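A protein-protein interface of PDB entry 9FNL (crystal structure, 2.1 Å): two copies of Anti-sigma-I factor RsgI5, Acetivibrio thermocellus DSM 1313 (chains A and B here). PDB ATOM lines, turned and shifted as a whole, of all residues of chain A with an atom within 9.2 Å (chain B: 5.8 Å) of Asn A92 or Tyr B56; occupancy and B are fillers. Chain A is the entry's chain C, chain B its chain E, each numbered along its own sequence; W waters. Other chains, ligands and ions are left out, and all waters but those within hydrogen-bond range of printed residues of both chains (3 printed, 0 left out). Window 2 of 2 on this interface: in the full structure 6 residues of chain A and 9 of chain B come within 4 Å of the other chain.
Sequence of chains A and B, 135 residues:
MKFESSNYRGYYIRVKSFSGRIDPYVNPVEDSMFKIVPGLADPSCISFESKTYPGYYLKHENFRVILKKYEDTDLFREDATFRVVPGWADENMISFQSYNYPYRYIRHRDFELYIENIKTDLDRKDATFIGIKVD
The backbone carbonyl oxygen of Phe B18 lies within hydrogen-bond range of the guanidinium group of Arg A9, at 2.7 Å.
The backbone carbonyl oxygen (O) of Leu B67 sits at hydrogen-bond distance from the guanidinium group (NH2) of Arg A9 (3.0 Å).
The side-chain carboxylate of Asp A90 sits at hydrogen-bond distance from the side-chain hydroxyl of Tyr B56, at 2.5 Å.
The side-chain amide nitrogen of Asn A92 lies within hydrogen-bond range of the side-chain hydroxyl of Tyr B56 (3.0 Å).
The backbone NH of Asn A92 sits at hydrogen-bond distance from the side-chain carboxylate of Asp A90 (2.8 Å).
The backbone NH (N) of Leu B67 lies within hydrogen-bond range of the backbone carbonyl oxygen (O) of Phe B18 (3.0 Å).
The side-chain hydroxyl of Ser B50 lies within hydrogen-bond range of the backbone NH of Tyr B53.
N of Ser B50 sits at hydrogen-bond distance from O of Tyr B56.
O of Lys B68 sits at hydrogen-bond distance from N of Tyr B57, at 2.9 Å.
Among the printed residues, pairs that only touch across the chains: Asn A92 with Tyr B53 (3.5 Å), Arg A9 with Lys B68 (3.8 Å) and Asn A92 with Phe B18 (3.9 Å).
Of the printed residues of chain B, Asn A92 touches Phe B18, Tyr B53 and Tyr B56.
Tyr B56 touches just these residues of chain A: Asp A90 and Asn A92.
No residue of chain A comes within 4 Å of Ser B50.
No residue of chain A comes within 4 Å of Gly B55.
Of the printed residues of chain A, Lys B68 touches Arg A9 (3.8 Å).
Of the printed residues of chain B, Arg A9 touches Phe B18 (2.7 Å), Leu B67 (3.0 Å) and Lys B68 (3.8 Å).
Of the printed residues of chain A, Leu B67 touches Arg A9 (3.0 Å).
The nearest printed residue of chain B that does not touch Asn A92 is Lys B69 (6.6 Å).
The nearest printed residue of chain A that does not touch Tyr B53 is Asp A90 (6.5 Å).
Printed residues of chain B that touch a printed residue of chain A: Phe B18, Tyr B53, Tyr B56, Leu B67 and Lys B68.
Hydrophobic or aromatic side chains of chain B within 4 Å of the printed part of chain A: Phe B18, Tyr B53 and Tyr B56.
Among the printed residues, 7 pairs touch across the chains.
Among the printed residues, no Asp or Glu carboxylate lies within 4 Å of a Lys or Arg side-chain nitrogen of the other chain.
No position is printed for both chains.
Of the 7 pairs that touch across the chains among the printed residues, none has its exchanged pair printed and touching as well.
Water W2 lies within hydrogen-bond range of NH1 of Arg A9 and O of Phe B18.
Water W1 bridges OH of Tyr B53 (2.6 Å) and O of Asn A92 (2.8 Å).
Water W3 lies within hydrogen-bond range of OH of Tyr B56 (2.9 Å), OE1 of Glu A91 (3.3 Å) and OD1 of Asp A90 (3.5 Å).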
ATOM      1  N   SER A   6     -13.634  -3.946 -35.534  1.00  0.00           N
ATOM      2  CA  SER A   6     -14.357  -4.587 -34.438  1.00  0.00           C
ATOM      3  C   SER A   6     -15.131  -5.823 -34.885  1.00  0.00           C
ATOM      4  O   SER A   6     -15.337  -6.736 -34.078  1.00  0.00           O
ATOM      5  CB  SER A   6     -15.325  -3.601 -33.789  1.00  0.00           C
ATOM      6  OG  SER A   6     -16.392  -3.290 -34.675  1.00  0.00           O
ATOM      7  N   ARG A   9     -12.194  -8.989 -36.271  1.00  0.00           N
ATOM      8  CA  ARG A   9     -11.037  -8.910 -35.389  1.00  0.00           C
ATOM      9  C   ARG A   9      -9.824  -9.544 -36.062  1.00  0.00           C
ATOM     10  O   ARG A   9      -9.938 -10.560 -36.754  1.00  0.00           O
ATOM     11  CB  ARG A   9     -11.336  -9.603 -34.055  1.00  0.00           C
ATOM     12  CG  ARG A   9     -12.483  -8.971 -33.275  1.00  0.00           C
ATOM     13  CD  ARG A   9     -12.144  -7.544 -32.849  1.00  0.00           C
ATOM     14  NE  ARG A   9     -11.020  -7.537 -31.922  1.00  0.00           N
ATOM     15  CZ  ARG A   9     -11.137  -7.626 -30.601  1.00  0.00           C
ATOM     16  NH1 ARG A   9     -10.054  -7.633 -29.853  1.00  0.00           N
ATOM     17  NH2 ARG A   9     -12.337  -7.693 -30.029  1.00  0.00           N
ATOM     18  N   VAL A  85     -15.012   9.776 -32.622  1.00  0.00           N
ATOM     19  CA  VAL A  85     -16.246   9.764 -31.834  1.00  0.00           C
ATOM     20  C   VAL A  85     -16.421   8.375 -31.233  1.00  0.00           C
ATOM     21  O   VAL A  85     -15.787   7.407 -31.683  1.00  0.00           O
ATOM     22  CB  VAL A  85     -17.469  10.159 -32.691  1.00  0.00           C
ATOM     23  CG1 VAL A  85     -17.266  11.540 -33.264  1.00  0.00           C
ATOM     24  CG2 VAL A  85     -17.709   9.139 -33.792  1.00  0.00           C
ATOM     25  N   PRO A  86     -17.270   8.241 -30.208  1.00  0.00           N
ATOM     26  CA  PRO A  86     -17.579   6.902 -29.687  1.00  0.00           C
ATOM     27  C   PRO A  86     -18.034   5.977 -30.807  1.00  0.00           C
ATOM     28  O   PRO A  86     -18.773   6.380 -31.707  1.00  0.00           O
ATOM     29  CB  PRO A  86     -18.708   7.162 -28.679  1.00  0.00           C
ATOM     30  CG  PRO A  86     -18.487   8.564 -28.227  1.00  0.00           C
ATOM     31  CD  PRO A  86     -17.972   9.296 -29.451  1.00  0.00           C
ATOM     32  N   GLY A  87     -17.589   4.725 -30.742  1.00  0.00           N
ATOM     33  CA  GLY A  87     -17.876   3.794 -31.821  1.00  0.00           C
ATOM     34  C   GLY A  87     -19.369   3.597 -32.023  1.00  0.00           C
ATOM     35  O   GLY A  87     -20.137   3.503 -31.065  1.00  0.00           O
ATOM     36  N   TRP A  88     -19.772   3.520 -33.297  1.00  0.00           N
ATOM     37  CA  TRP A  88     -21.181   3.354 -33.653  1.00  0.00           C
ATOM     38  C   TRP A  88     -21.783   2.084 -33.060  1.00  0.00           C
ATOM     39  O   TRP A  88     -22.942   2.084 -32.637  1.00  0.00           O
ATOM     40  CB  TRP A  88     -21.337   3.316 -35.169  1.00  0.00           C
ATOM     41  CG  TRP A  88     -21.568   4.640 -35.802  1.00  0.00           C
ATOM     42  CD1 TRP A  88     -20.667   5.379 -36.510  1.00  0.00           C
ATOM     43  CD2 TRP A  88     -22.790   5.383 -35.805  1.00  0.00           C
ATOM     44  NE1 TRP A  88     -21.252   6.544 -36.955  1.00  0.00           N
ATOM     45  CE2 TRP A  88     -22.556   6.569 -36.536  1.00  0.00           C
ATOM     46  CE3 TRP A  88     -24.058   5.165 -35.257  1.00  0.00           C
ATOM     47  CZ2 TRP A  88     -23.544   7.531 -36.727  1.00  0.00           C
ATOM     48  CZ3 TRP A  88     -25.037   6.120 -35.449  1.00  0.00           C
ATOM     49  CH2 TRP A  88     -24.776   7.286 -36.184  1.00  0.00           C
ATOM     50  N   ALA A  89     -21.040   0.976 -33.080  1.00  0.00           N
ATOM     51  CA  ALA A  89     -21.549  -0.296 -32.583  1.00  0.00           C
ATOM     52  C   ALA A  89     -21.081  -0.602 -31.173  1.00  0.00           C
ATOM     53  O   ALA A  89     -21.463  -1.638 -30.614  1.00  0.00           O
ATOM     54  CB  ALA A  89     -21.141  -1.448 -33.513  1.00  0.00           C
ATOM     55  N   ASP A  90     -20.265   0.272 -30.588  1.00  0.00           N
ATOM     56  CA  ASP A  90     -19.698   0.035 -29.274  1.00  0.00           C
ATOM     57  C   ASP A  90     -19.021   1.300 -28.780  1.00  0.00           C
ATOM     58  O   ASP A  90     -17.950   1.681 -29.274  1.00  0.00           O
ATOM     59  CB  ASP A  90     -18.707  -1.130 -29.317  1.00  0.00           C
ATOM     60  CG  ASP A  90     -18.205  -1.524 -27.939  1.00  0.00           C
ATOM     61  OD1 ASP A  90     -18.191  -0.664 -27.031  1.00  0.00           O
ATOM     62  OD2 ASP A  90     -17.816  -2.706 -27.775  1.00  0.00           O
ATOM     63  N   GLU A  91     -19.635   1.925 -27.774  1.00  0.00           N
ATOM     64  CA  GLU A  91     -19.164   3.201 -27.254  1.00  0.00           C
ATOM     65  C   GLU A  91     -17.788   3.107 -26.625  1.00  0.00           C
ATOM     66  O   GLU A  91     -17.140   4.145 -26.447  1.00  0.00           O
ATOM     67  CB  GLU A  91     -20.154   3.743 -26.220  1.00  0.00           C
ATOM     68  CG  GLU A  91     -20.284   2.864 -24.978  1.00  0.00           C
ATOM     69  CD  GLU A  91     -21.446   1.878 -25.074  1.00  0.00           C
ATOM     70  OE1 GLU A  91     -21.660   1.297 -26.173  1.00  0.00           O
ATOM     71  OE2 GLU A  91     -22.142   1.685 -24.044  1.00  0.00           O
ATOM     72  N   ASN A  92     -17.337   1.899 -26.255  1.00  0.00           N
ATOM     73  CA  ASN A  92     -15.983   1.713 -25.751  1.00  0.00           C
ATOM     74  C   ASN A  92     -14.934   1.683 -26.853  1.00  0.00           C
ATOM     75  O   ASN A  92     -13.735   1.672 -26.545  1.00  0.00           O
ATOM     76  CB  ASN A  92     -15.914   0.428 -24.933  1.00  0.00           C
ATOM     77  CG  ASN A  92     -16.886   0.450 -23.789  1.00  0.00           C
ATOM     78  OD1 ASN A  92     -16.872   1.382 -22.991  1.00  0.00           O
ATOM     79  ND2 ASN A  92     -17.772  -0.542 -23.728  1.00  0.00           N
ATOM     80  N   MET A  93     -15.355   1.660 -28.116  1.00  0.00           N
ATOM     81  CA  MET A  93     -14.474   1.684 -29.278  1.00  0.00           C
ATOM     82  C   MET A  93     -14.644   3.034 -29.982  1.00  0.00           C
ATOM     83  O   MET A  93     -15.217   3.974 -29.416  1.00  0.00           O
ATOM     84  CB  MET A  93     -14.769   0.479 -30.183  1.00  0.00           C
ATOM     85  CG  MET A  93     -14.484  -0.868 -29.497  1.00  0.00           C
ATOM     86  SD  MET A  93     -15.034  -2.306 -30.435  1.00  0.00           S
ATOM     87  CE  MET A  93     -14.548  -3.631 -29.310  1.00  0.00           C
ATOM     88  N   ILE A  94     -14.142   3.147 -31.218  1.00  0.00           N
ATOM     89  CA  ILE A  94     -14.124   4.447 -31.875  1.00  0.00           C
ATOM     90  C   ILE A  94     -14.619   4.344 -33.314  1.00  0.00           C
ATOM     91  O   ILE A  94     -14.555   3.295 -33.958  1.00  0.00           O
ATOM     92  CB  ILE A  94     -12.723   5.115 -31.842  1.00  0.00           C
ATOM     93  CG1 ILE A  94     -11.704   4.300 -32.636  1.00  0.00           C
ATOM     94  CG2 ILE A  94     -12.253   5.374 -30.414  1.00  0.00           C
ATOM     95  CD1 ILE A  94     -10.286   4.849 -32.544  1.00  0.00           C
ATOM     96  N   SER A  95     -15.141   5.469 -33.802  1.00  0.00           N
ATOM     97  CA  SER A  95     -15.463   5.693 -35.199  1.00  0.00           C
ATOM     98  C   SER A  95     -14.847   7.014 -35.644  1.00  0.00           C
ATOM     99  O   SER A  95     -14.380   7.824 -34.836  1.00  0.00           O
ATOM    100  CB  SER A  95     -16.977   5.687 -35.449  1.00  0.00           C
ATOM    101  OG  SER A  95     -17.581   4.486 -35.001  1.00  0.00           O
ATOM    102  N   THR A 128     -16.852   0.686 -36.840  1.00  0.00           N
ATOM    103  CA  THR A 128     -16.357   0.684 -35.474  1.00  0.00           C
ATOM    104  C   THR A 128     -15.008  -0.019 -35.427  1.00  0.00           C
ATOM    105  O   THR A 128     -14.868  -1.142 -35.927  1.00  0.00           O
ATOM    106  CB  THR A 128     -17.361   0.022 -34.541  1.00  0.00           C
ATOM    107  OG1 THR A 128     -18.581   0.766 -34.590  1.00  0.00           O
ATOM    108  CG2 THR A 128     -16.831  -0.015 -33.089  1.00  0.00           C
ATOM    109  N   PHE A 129     -14.026   0.655 -34.838  1.00  0.00           N
ATOM    110  CA  PHE A 129     -12.634   0.251 -34.880  1.00  0.00           C
ATOM    111  C   PHE A 129     -12.035   0.340 -33.482  1.00  0.00           C
ATOM    112  O   PHE A 129     -12.581   0.995 -32.589  1.00  0.00           O
ATOM    113  CB  PHE A 129     -11.818   1.130 -35.859  1.00  0.00           C
ATOM    114  CG  PHE A 129     -12.242   0.991 -37.309  1.00  0.00           C
ATOM    115  CD1 PHE A 129     -11.721  -0.025 -38.111  1.00  0.00           C
ATOM    116  CD2 PHE A 129     -13.166   1.868 -37.863  1.00  0.00           C
ATOM    117  CE1 PHE A 129     -12.113  -0.164 -39.427  1.00  0.00           C
ATOM    118  CE2 PHE A 129     -13.567   1.741 -39.198  1.00  0.00           C
ATOM    119  CZ  PHE A 129     -13.038   0.725 -39.979  1.00  0.00           C
ATOM    120  N   ILE A 130     -10.890  -0.317 -33.320  1.00  0.00           N
ATOM    121  CA  ILE A 130     -10.135  -0.367 -32.070  1.00  0.00           C
ATOM    122  C   ILE A 130      -8.799   0.310 -32.327  1.00  0.00           C
ATOM    123  O   ILE A 130      -8.034  -0.136 -33.187  1.00  0.00           O
ATOM    124  CB  ILE A 130      -9.918  -1.817 -31.591  1.00  0.00           C
ATOM    125  CG1 ILE A 130     -11.250  -2.510 -31.282  1.00  0.00           C
ATOM    126  CG2 ILE A 130      -8.988  -1.860 -30.371  1.00  0.00           C
ATOM    127  CD1 ILE A 130     -11.164  -4.029 -31.312  1.00  0.00           C
ATOM    128  N   GLY A 131      -8.515   1.383 -31.589  1.00  0.00           N
ATOM    129  CA  GLY A 131      -7.216   2.029 -31.690  1.00  0.00           C
ATOM    130  C   GLY A 131      -6.169   1.248 -30.912  1.00  0.00           C
ATOM    131  O   GLY A 131      -6.406   0.836 -29.770  1.00  0.00           O
ATOM    132  N   PHE B  18      -8.373  -4.287 -26.073  1.00  0.00           N
ATOM    133  CA  PHE B  18      -9.243  -5.444 -26.271  1.00  0.00           C
ATOM    134  C   PHE B  18      -8.484  -6.694 -26.725  1.00  0.00           C
ATOM    135  O   PHE B  18      -9.083  -7.609 -27.299  1.00  0.00           O
ATOM    136  CB  PHE B  18     -10.382  -5.114 -27.247  1.00  0.00           C
ATOM    137  CG  PHE B  18     -11.291  -4.042 -26.743  1.00  0.00           C
ATOM    138  CD1 PHE B  18     -12.386  -4.362 -25.957  1.00  0.00           C
ATOM    139  CD2 PHE B  18     -11.031  -2.707 -27.017  1.00  0.00           C
ATOM    140  CE1 PHE B  18     -13.212  -3.382 -25.476  1.00  0.00           C
ATOM    141  CE2 PHE B  18     -11.855  -1.724 -26.536  1.00  0.00           C
ATOM    142  CZ  PHE B  18     -12.947  -2.056 -25.762  1.00  0.00           C
ATOM    143  N   PHE B  48     -13.811 -15.834 -18.180  1.00  0.00           N
ATOM    144  CA  PHE B  48     -13.189 -14.640 -17.603  1.00  0.00           C
ATOM    145  C   PHE B  48     -13.985 -13.422 -18.037  1.00  0.00           C
ATOM    146  O   PHE B  48     -13.893 -13.008 -19.196  1.00  0.00           O
ATOM    147  CB  PHE B  48     -11.744 -14.467 -18.074  1.00  0.00           C
ATOM    148  CG  PHE B  48     -10.839 -15.643 -17.813  1.00  0.00           C
ATOM    149  CD1 PHE B  48     -10.830 -16.737 -18.661  1.00  0.00           C
ATOM    150  CD2 PHE B  48      -9.938 -15.613 -16.758  1.00  0.00           C
ATOM    151  CE1 PHE B  48      -9.966 -17.804 -18.441  1.00  0.00           C
ATOM    152  CE2 PHE B  48      -9.071 -16.665 -16.534  1.00  0.00           C
ATOM    153  CZ  PHE B  48      -9.079 -17.763 -17.375  1.00  0.00           C
ATOM    154  N   GLU B  49     -14.724 -12.811 -17.113  1.00  0.00           N
ATOM    155  CA  GLU B  49     -15.440 -11.584 -17.431  1.00  0.00           C
ATOM    156  C   GLU B  49     -14.620 -10.348 -17.059  1.00  0.00           C
ATOM    157  O   GLU B  49     -14.019 -10.284 -15.986  1.00  0.00           O
ATOM    158  CB  GLU B  49     -16.797 -11.541 -16.722  1.00  0.00           C
ATOM    159  CG  GLU B  49     -17.671 -10.398 -17.243  1.00  0.00           C
ATOM    160  CD  GLU B  49     -19.003 -10.279 -16.523  1.00  0.00           C
ATOM    161  OE1 GLU B  49     -19.232 -11.032 -15.550  1.00  0.00           O
ATOM    162  OE2 GLU B  49     -19.818  -9.424 -16.927  1.00  0.00           O
ATOM    163  N   SER B  50     -14.624  -9.353 -17.939  1.00  0.00           N
ATOM    164  CA  SER B  50     -13.869  -8.134 -17.678  1.00  0.00           C
ATOM    165  C   SER B  50     -14.469  -7.366 -16.506  1.00  0.00           C
ATOM    166  O   SER B  50     -15.687  -7.170 -16.424  1.00  0.00           O
ATOM    167  CB  SER B  50     -13.855  -7.239 -18.918  1.00  0.00           C
ATOM    168  OG  SER B  50     -13.274  -5.983 -18.623  1.00  0.00           O
ATOM    169  N   TYR B  53     -15.036  -3.808 -18.233  1.00  0.00           N
ATOM    170  CA  TYR B  53     -16.093  -3.829 -19.239  1.00  0.00           C
ATOM    171  C   TYR B  53     -17.044  -4.974 -18.913  1.00  0.00           C
ATOM    172  O   TYR B  53     -16.902  -6.079 -19.461  1.00  0.00           O
ATOM    173  CB  TYR B  53     -15.513  -4.004 -20.640  1.00  0.00           C
ATOM    174  CG  TYR B  53     -14.551  -2.922 -21.085  1.00  0.00           C
ATOM    175  CD1 TYR B  53     -15.015  -1.675 -21.501  1.00  0.00           C
ATOM    176  CD2 TYR B  53     -13.182  -3.157 -21.121  1.00  0.00           C
ATOM    177  CE1 TYR B  53     -14.134  -0.684 -21.926  1.00  0.00           C
ATOM    178  CE2 TYR B  53     -12.290  -2.176 -21.551  1.00  0.00           C
ATOM    179  CZ  TYR B  53     -12.773  -0.945 -21.953  1.00  0.00           C
ATOM    180  OH  TYR B  53     -11.892   0.027 -22.373  1.00  0.00           O
ATOM    181  N   PRO B  54     -18.009  -4.760 -18.019  1.00  0.00           N
ATOM    182  CA  PRO B  54     -18.965  -5.829 -17.710  1.00  0.00           C
ATOM    183  C   PRO B  54     -19.624  -6.335 -18.984  1.00  0.00           C
ATOM    184  O   PRO B  54     -19.855  -5.581 -19.935  1.00  0.00           O
ATOM    185  CB  PRO B  54     -19.970  -5.150 -16.771  1.00  0.00           C
ATOM    186  CG  PRO B  54     -19.206  -4.012 -16.153  1.00  0.00           C
ATOM    187  CD  PRO B  54     -18.235  -3.546 -17.210  1.00  0.00           C
ATOM    188  N   GLY B  55     -19.886  -7.639 -19.018  1.00  0.00           N
ATOM    189  CA  GLY B  55     -20.454  -8.250 -20.197  1.00  0.00           C
ATOM    190  C   GLY B  55     -19.485  -8.473 -21.336  1.00  0.00           C
ATOM    191  O   GLY B  55     -19.927  -8.822 -22.430  1.00  0.00           O
ATOM    192  N   TYR B  56     -18.186  -8.265 -21.123  1.00  0.00           N
ATOM    193  CA  TYR B  56     -17.148  -8.608 -22.090  1.00  0.00           C
ATOM    194  C   TYR B  56     -16.349  -9.778 -21.542  1.00  0.00           C
ATOM    195  O   TYR B  56     -16.072  -9.835 -20.343  1.00  0.00           O
ATOM    196  CB  TYR B  56     -16.194  -7.440 -22.359  1.00  0.00           C
ATOM    197  CG  TYR B  56     -16.763  -6.280 -23.169  1.00  0.00           C
ATOM    198  CD1 TYR B  56     -17.895  -5.598 -22.746  1.00  0.00           C
ATOM    199  CD2 TYR B  56     -16.146  -5.857 -24.347  1.00  0.00           C
ATOM    200  CE1 TYR B  56     -18.409  -4.526 -23.463  1.00  0.00           C
ATOM    201  CE2 TYR B  56     -16.659  -4.768 -25.080  1.00  0.00           C
ATOM    202  CZ  TYR B  56     -17.788  -4.117 -24.626  1.00  0.00           C
ATOM    203  OH  TYR B  56     -18.318  -3.054 -25.322  1.00  0.00           O
ATOM    204  N   TYR B  57     -15.947 -10.691 -22.418  1.00  0.00           N
ATOM    205  CA  TYR B  57     -15.300 -11.913 -21.978  1.00  0.00           C
ATOM    206  C   TYR B  57     -14.030 -12.155 -22.774  1.00  0.00           C
ATOM    207  O   TYR B  57     -13.969 -11.849 -23.971  1.00  0.00           O
ATOM    208  CB  TYR B  57     -16.242 -13.104 -22.130  1.00  0.00           C
ATOM    209  CG  TYR B  57     -17.426 -13.033 -21.206  1.00  0.00           C
ATOM    210  CD1 TYR B  57     -18.562 -12.312 -21.550  1.00  0.00           C
ATOM    211  CD2 TYR B  57     -17.410 -13.691 -19.984  1.00  0.00           C
ATOM    212  CE1 TYR B  57     -19.647 -12.252 -20.709  1.00  0.00           C
ATOM    213  CE2 TYR B  57     -18.500 -13.629 -19.120  1.00  0.00           C
ATOM    214  CZ  TYR B  57     -19.608 -12.916 -19.487  1.00  0.00           C
ATOM    215  OH  TYR B  57     -20.685 -12.860 -18.633  1.00  0.00           O
ATOM    216  N   LEU B  58     -13.012 -12.693 -22.097  1.00  0.00           N
ATOM    217  CA  LEU B  58     -11.881 -13.276 -22.809  1.00  0.00           C
ATOM    218  C   LEU B  58     -12.377 -14.443 -23.652  1.00  0.00           C
ATOM    219  O   LEU B  58     -13.159 -15.272 -23.177  1.00  0.00           O
ATOM    220  CB  LEU B  58     -10.808 -13.761 -21.826  1.00  0.00           C
ATOM    221  CG  LEU B  58     -10.083 -12.711 -20.986  1.00  0.00           C
ATOM    222  CD1 LEU B  58      -8.940 -13.349 -20.229  1.00  0.00           C
ATOM    223  CD2 LEU B  58      -9.555 -11.609 -21.882  1.00  0.00           C
ATOM    224  N   LEU B  67     -10.522  -9.805 -25.939  1.00  0.00           N
ATOM    225  CA  LEU B  67     -11.702  -9.417 -25.185  1.00  0.00           C
ATOM    226  C   LEU B  67     -12.790  -9.033 -26.172  1.00  0.00           C
ATOM    227  O   LEU B  67     -12.547  -8.247 -27.092  1.00  0.00           O
ATOM    228  CB  LEU B  67     -11.416  -8.248 -24.237  1.00  0.00           C
ATOM    229  CG  LEU B  67     -12.563  -8.015 -23.245  1.00  0.00           C
ATOM    230  CD1 LEU B  67     -12.516  -9.093 -22.184  1.00  0.00           C
ATOM    231  CD2 LEU B  67     -12.523  -6.636 -22.609  1.00  0.00           C
ATOM    232  N   LYS B  68     -13.985  -9.563 -25.965  1.00  0.00           N
ATOM    233  CA  LYS B  68     -15.075  -9.338 -26.895  1.00  0.00           C
ATOM    234  C   LYS B  68     -16.376  -9.254 -26.122  1.00  0.00           C
ATOM    235  O   LYS B  68     -16.555  -9.961 -25.131  1.00  0.00           O
ATOM    236  CB  LYS B  68     -15.148 -10.466 -27.930  1.00  0.00           C
ATOM    237  CG  LYS B  68     -15.330  -9.979 -29.342  1.00  0.00           C
ATOM    238  CD  LYS B  68     -15.455 -11.140 -30.321  1.00  0.00           C
ATOM    239  CE  LYS B  68     -15.739 -10.609 -31.712  1.00  0.00           C
ATOM    240  NZ  LYS B  68     -16.154 -11.667 -32.668  1.00  0.00           N
ATOM    241  N   LYS B  69     -17.277  -8.381 -26.578  1.00  0.00           N
ATOM    242  CA  LYS B  69     -18.579  -8.264 -25.946  1.00  0.00           C
ATOM    243  C   LYS B  69     -19.355  -9.554 -26.157  1.00  0.00           C
ATOM    244  O   LYS B  69     -19.290 -10.157 -27.227  1.00  0.00           O
ATOM    245  CB  LYS B  69     -19.339  -7.070 -26.533  1.00  0.00           C
ATOM    246  CG  LYS B  69     -20.667  -6.751 -25.867  1.00  0.00           C
ATOM    247  CD  LYS B  69     -21.266  -5.464 -26.473  1.00  0.00           C
ATOM    248  CE  LYS B  69     -22.515  -5.009 -25.731  1.00  0.00           C
ATOM    249  NZ  LYS B  69     -23.561  -4.510 -26.677  1.00  0.00           N
ATOM    250  N   TYR B  70     -20.081  -9.982 -25.124  1.00  0.00           N
ATOM    251  CA  TYR B  70     -20.842 -11.228 -25.202  1.00  0.00           C
ATOM    252  C   TYR B  70     -21.696 -11.266 -26.465  1.00  0.00           C
ATOM    253  O   TYR B  70     -22.271 -10.255 -26.869  1.00  0.00           O
ATOM    254  CB  TYR B  70     -21.736 -11.389 -23.976  1.00  0.00           C
ATOM    255  CG  TYR B  70     -22.624 -12.616 -24.037  1.00  0.00           C
ATOM    256  CD1 TYR B  70     -22.133 -13.867 -23.689  1.00  0.00           C
ATOM    257  CD2 TYR B  70     -23.954 -12.522 -24.438  1.00  0.00           C
ATOM    258  CE1 TYR B  70     -22.936 -14.994 -23.736  1.00  0.00           C
ATOM    259  CE2 TYR B  70     -24.764 -13.643 -24.489  1.00  0.00           C
ATOM    260  CZ  TYR B  70     -24.243 -14.879 -24.138  1.00  0.00           C
ATOM    261  OH  TYR B  70     -25.030 -16.002 -24.183  1.00  0.00           O
HETATM  262  O   HOH W   1     -12.500   1.985 -24.051  1.00  0.00           O
HETATM  263  O   HOH W   2      -7.731  -6.456 -29.816  1.00  0.00           O
HETATM  264  O   HOH W   3     -20.876  -1.773 -25.143  1.00  0.00           O
